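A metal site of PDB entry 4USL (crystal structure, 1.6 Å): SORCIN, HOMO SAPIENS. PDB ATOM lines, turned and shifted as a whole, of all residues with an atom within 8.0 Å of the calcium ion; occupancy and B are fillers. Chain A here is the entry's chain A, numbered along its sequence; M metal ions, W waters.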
ATOM      1  N   PHE A  39       7.093   1.559  22.334  1.00  0.00           N
ATOM      2  CA  PHE A  39       6.851   0.862  21.053  1.00  0.00           C
ATOM      3  C   PHE A  39       5.442   0.279  20.978  1.00  0.00           C
ATOM      4  O   PHE A  39       4.697   0.490  20.003  1.00  0.00           O
ATOM      5  CB  PHE A  39       7.864  -0.278  20.824  1.00  0.00           C
ATOM      6  CG  PHE A  39       7.472  -1.189  19.692  1.00  0.00           C
ATOM      7  CD1 PHE A  39       7.613  -0.799  18.366  1.00  0.00           C
ATOM      8  CD2 PHE A  39       6.827  -2.422  19.954  1.00  0.00           C
ATOM      9  CE1 PHE A  39       7.182  -1.619  17.330  1.00  0.00           C
ATOM     10  CE2 PHE A  39       6.404  -3.230  18.920  1.00  0.00           C
ATOM     11  CZ  PHE A  39       6.576  -2.836  17.600  1.00  0.00           C
ATOM     12  N   ALA A  40       5.065  -0.492  22.000  1.00  0.00           N
ATOM     13  CA  ALA A  40       3.768  -1.179  21.975  1.00  0.00           C
ATOM     14  C   ALA A  40       2.571  -0.217  21.936  1.00  0.00           C
ATOM     15  O   ALA A  40       1.579  -0.490  21.270  1.00  0.00           O
ATOM     16  CB  ALA A  40       3.655  -2.145  23.129  1.00  0.00           C
ATOM     17  N   ALA A  41       2.679   0.918  22.625  1.00  0.00           N
ATOM     18  CA  ALA A  41       1.620   1.926  22.610  1.00  0.00           C
ATOM     19  C   ALA A  41       1.447   2.554  21.230  1.00  0.00           C
ATOM     20  O   ALA A  41       0.326   2.812  20.771  1.00  0.00           O
ATOM     21  CB  ALA A  41       1.893   2.994  23.661  1.00  0.00           C
ATOM     22  N   VAL A  42       2.571   2.811  20.582  1.00  0.00           N
ATOM     23  CA  VAL A  42       2.558   3.375  19.234  1.00  0.00           C
ATOM     24  C   VAL A  42       2.009   2.352  18.242  1.00  0.00           C
ATOM     25  O   VAL A  42       1.212   2.686  17.333  1.00  0.00           O
ATOM     26  CB  VAL A  42       3.978   3.840  18.830  1.00  0.00           C
ATOM     27  CG1 VAL A  42       3.996   4.343  17.385  1.00  0.00           C
ATOM     28  CG2 VAL A  42       4.481   4.922  19.753  1.00  0.00           C
ATOM     29  N   ALA A  43       2.439   1.102  18.397  1.00  0.00           N
ATOM     30  CA  ALA A  43       2.053   0.025  17.472  1.00  0.00           C
ATOM     31  C   ALA A  43       0.592  -0.326  17.542  1.00  0.00           C
ATOM     32  O   ALA A  43      -0.003  -0.637  16.552  1.00  0.00           O
ATOM     33  CB  ALA A  43       2.858  -1.219  17.748  1.00  0.00           C
ATOM     34  N   GLY A  44       0.024  -0.290  18.727  1.00  0.00           N
ATOM     35  CA  GLY A  44      -1.380  -0.604  18.870  1.00  0.00           C
ATOM     36  C   GLY A  44      -1.686  -2.056  18.545  1.00  0.00           C
ATOM     37  O   GLY A  44      -0.843  -2.948  18.733  1.00  0.00           O
ATOM     38  N   GLN A  45      -2.896  -2.265  18.017  1.00  0.00           N
ATOM     39  CA  GLN A  45      -3.540  -3.589  17.956  1.00  0.00           C
ATOM     40  C   GLN A  45      -2.782  -4.681  17.219  1.00  0.00           C
ATOM     41  O   GLN A  45      -2.718  -5.809  17.695  1.00  0.00           O
ATOM     42  CB  GLN A  45      -4.927  -3.441  17.328  1.00  0.00           C
ATOM     43  CG  GLN A  45      -5.818  -4.683  17.406  1.00  0.00           C
ATOM     44  CD  GLN A  45      -7.212  -4.428  16.853  1.00  0.00           C
ATOM     45  OE1 GLN A  45      -7.775  -3.338  17.047  1.00  0.00           O
ATOM     46  NE2 GLN A  45      -7.783  -5.420  16.164  1.00  0.00           N
ATOM     47  N   ASP A  46      -2.205  -4.362  16.061  1.00  0.00           N
ATOM     48  CA  ASP A  46      -1.486  -5.376  15.278  1.00  0.00           C
ATOM     49  C   ASP A  46      -0.018  -5.596  15.662  1.00  0.00           C
ATOM     50  O   ASP A  46       0.651  -6.419  15.061  1.00  0.00           O
ATOM     51  CB  ASP A  46      -1.647  -5.145  13.764  1.00  0.00           C
ATOM     52  CG  ASP A  46      -0.941  -3.882  13.252  1.00  0.00           C
ATOM     53  OD1 ASP A  46      -0.331  -3.155  14.063  1.00  0.00           O
ATOM     54  OD2 ASP A  46      -1.039  -3.628  12.035  1.00  0.00           O
ATOM     55  N   GLY A  47       0.470  -4.864  16.674  1.00  0.00           N
ATOM     56  CA  GLY A  47       1.829  -5.024  17.167  1.00  0.00           C
ATOM     57  C   GLY A  47       2.934  -4.555  16.194  1.00  0.00           C
ATOM     58  O   GLY A  47       4.107  -4.892  16.357  1.00  0.00           O
ATOM     59  N   GLN A  48       2.531  -3.810  15.159  1.00  0.00           N
ATOM     60  CA  GLN A  48       3.476  -3.237  14.180  1.00  0.00           C
ATOM     61  C   GLN A  48       3.174  -1.762  14.016  1.00  0.00           C
ATOM     62  O   GLN A  48       2.022  -1.321  14.150  1.00  0.00           O
ATOM     63  CB  GLN A  48       3.336  -3.923  12.814  1.00  0.00           C
ATOM     64  CG  GLN A  48       3.725  -5.406  12.804  1.00  0.00           C
ATOM     65  CD  GLN A  48       5.227  -5.655  12.988  1.00  0.00           C
ATOM     66  OE1 GLN A  48       5.632  -6.448  13.869  1.00  0.00           O
ATOM     67  NE2 GLN A  48       6.067  -5.000  12.187  1.00  0.00           N
ATOM     68  N   ILE A  49       4.212  -1.009  13.659  1.00  0.00           N
ATOM     69  CA  ILE A  49       4.049   0.436  13.444  1.00  0.00           C
ATOM     70  C   ILE A  49       3.927   0.682  11.937  1.00  0.00           C
ATOM     71  O   ILE A  49       4.807   0.301  11.172  1.00  0.00           O
ATOM     72  CB  ILE A  49       5.207   1.242  14.074  1.00  0.00           C
ATOM     73  CG1 ILE A  49       5.132   1.155  15.620  1.00  0.00           C
ATOM     74  CG2 ILE A  49       5.194   2.714  13.618  1.00  0.00           C
ATOM     75  CD1 ILE A  49       6.348   1.646  16.339  1.00  0.00           C
ATOM     76  N   ASP A  50       2.855   1.349  11.538  1.00  0.00           N
ATOM     77  CA  ASP A  50       2.740   1.850  10.145  1.00  0.00           C
ATOM     78  C   ASP A  50       3.128   3.330  10.078  1.00  0.00           C
ATOM     79  O   ASP A  50       3.343   3.961  11.119  1.00  0.00           O
ATOM     80  CB  ASP A  50       1.341   1.563   9.571  1.00  0.00           C
ATOM     81  CG  ASP A  50       0.231   2.304  10.287  1.00  0.00           C
ATOM     82  OD1 ASP A  50       0.386   3.496  10.615  1.00  0.00           O
ATOM     83  OD2 ASP A  50      -0.827   1.693  10.496  1.00  0.00           O
ATOM     84  N   ALA A  51       3.219   3.893   8.878  1.00  0.00           N
ATOM     85  CA  ALA A  51       3.752   5.260   8.763  1.00  0.00           C
ATOM     86  C   ALA A  51       2.832   6.296   9.416  1.00  0.00           C
ATOM     87  O   ALA A  51       3.292   7.324   9.870  1.00  0.00           O
ATOM     88  CB  ALA A  51       4.031   5.623   7.325  1.00  0.00           C
ATOM     89  N   GLU A  53       0.920   5.770  12.153  1.00  0.00           N
ATOM     90  CA  GLU A  53       1.257   5.665  13.572  1.00  0.00           C
ATOM     91  C   GLU A  53       2.592   6.338  13.914  1.00  0.00           C
ATOM     92  O   GLU A  53       2.724   7.035  14.910  1.00  0.00           O
ATOM     93  CB  GLU A  53       1.288   4.200  14.013  1.00  0.00           C
ATOM     94  CG  GLU A  53      -0.100   3.611  14.049  1.00  0.00           C
ATOM     95  CD  GLU A  53      -0.157   2.092  14.101  1.00  0.00           C
ATOM     96  OE1 GLU A  53       0.825   1.402  13.703  1.00  0.00           O
ATOM     97  OE2 GLU A  53      -1.219   1.553  14.541  1.00  0.00           O
ATOM     98  N   LEU A  54       3.602   6.087  13.072  1.00  0.00           N
ATOM     99  CA  LEU A  54       4.894   6.740  13.224  1.00  0.00           C
ATOM    100  C   LEU A  54       4.800   8.255  13.153  1.00  0.00           C
ATOM    101  O   LEU A  54       5.428   8.938  13.950  1.00  0.00           O
ATOM    102  CB  LEU A  54       5.946   6.217  12.207  1.00  0.00           C
ATOM    103  CG  LEU A  54       7.404   6.646  12.488  1.00  0.00           C
ATOM    104  CD1 LEU A  54       7.929   6.258  13.872  1.00  0.00           C
ATOM    105  CD2 LEU A  54       8.310   6.080  11.393  1.00  0.00           C
ATOM    106  N   ARG A  56       2.275  10.185  13.921  1.00  0.00           N
ATOM    107  CA  ARG A  56       1.691  10.649  15.170  1.00  0.00           C
ATOM    108  C   ARG A  56       2.762  10.615  16.284  1.00  0.00           C
ATOM    109  O   ARG A  56       2.957  11.559  17.020  1.00  0.00           O
ATOM    110  CB  ARG A  56       0.445   9.776  15.446  1.00  0.00           C
ATOM    111  CG  ARG A  56      -0.680  10.369  16.230  1.00  0.00           C
ATOM    112  CD  ARG A  56      -1.860   9.409  16.316  1.00  0.00           C
ATOM    113  NE  ARG A  56      -2.207   8.793  15.045  1.00  0.00           N
ATOM    114  CZ  ARG A  56      -2.312   7.487  14.779  1.00  0.00           C
ATOM    115  NH1 ARG A  56      -2.140   6.537  15.705  1.00  0.00           N
ATOM    116  NH2 ARG A  56      -2.634   7.116  13.551  1.00  0.00           N
ATOM    117  N   THR A  89       6.191  -2.627   7.413  1.00  0.00           N
ATOM    118  CA  THR A  89       5.766  -2.089   8.702  1.00  0.00           C
ATOM    119  C   THR A  89       6.971  -2.140   9.601  1.00  0.00           C
ATOM    120  O   THR A  89       7.891  -2.918   9.370  1.00  0.00           O
ATOM    121  CB  THR A  89       4.664  -2.969   9.333  1.00  0.00           C
ATOM    122  OG1 THR A  89       5.177  -4.279   9.617  1.00  0.00           O
ATOM    123  CG2 THR A  89       3.488  -3.047   8.416  1.00  0.00           C
ATOM    124  N   MET A  90       6.930  -1.362  10.686  1.00  0.00           N
ATOM    125  CA  MET A  90       8.037  -1.254  11.612  1.00  0.00           C
ATOM    126  C   MET A  90       7.836  -2.052  12.918  1.00  0.00           C
ATOM    127  O   MET A  90       6.894  -1.771  13.709  1.00  0.00           O
ATOM    128  CB  MET A  90       8.270   0.236  11.906  1.00  0.00           C
ATOM    129  CG  MET A  90       9.207   0.553  13.056  1.00  0.00           C
ATOM    130  SD  MET A  90       9.629   2.315  13.148  1.00  0.00           S
ATOM    131  CE  MET A  90      10.761   2.490  11.803  1.00  0.00           C
HETATM  132 CA    CA M   1      -0.218  -0.801  14.221  1.00  0.00          CA
HETATM  133  O   HOH W   1      -0.726  -0.815  11.851  1.00  0.00           O
HETATM  134  O   HOH W   2      -2.569  -1.321  14.709  1.00  0.00           O
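NE2 of Gln 48 sits at hydrogen-bond distance from OG1 of Thr 89, 2.8 Å away.
The backbone NH (N) of Glu 53 is in hydrogen-bond range of the side-chain carboxylate (OD1) of Asp 50, at 2.8 Å.
Within 4 Å of the calcium ion: Ala 43, Asp 46, Gln 48 and Glu 53.
The nearest printed residue that does not touch the calcium ion is Ile 49 (4.5 Å).
The calcium ion is bound by O of Gln 48 (2.3 Å), O of Ala 43 (2.3 Å), OD1 of Asp 46 (2.4 Å), water W1 (2.4 Å), water W2 (2.5 Å), OE1 of Glu 53 (2.5 Å) and OE2 of Glu 53 (2.6 Å).
The calcium ion has seven donor atoms within binding distance.
Water W1 bridges OD2 of Asp 46 and OD2 of Asp 50.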
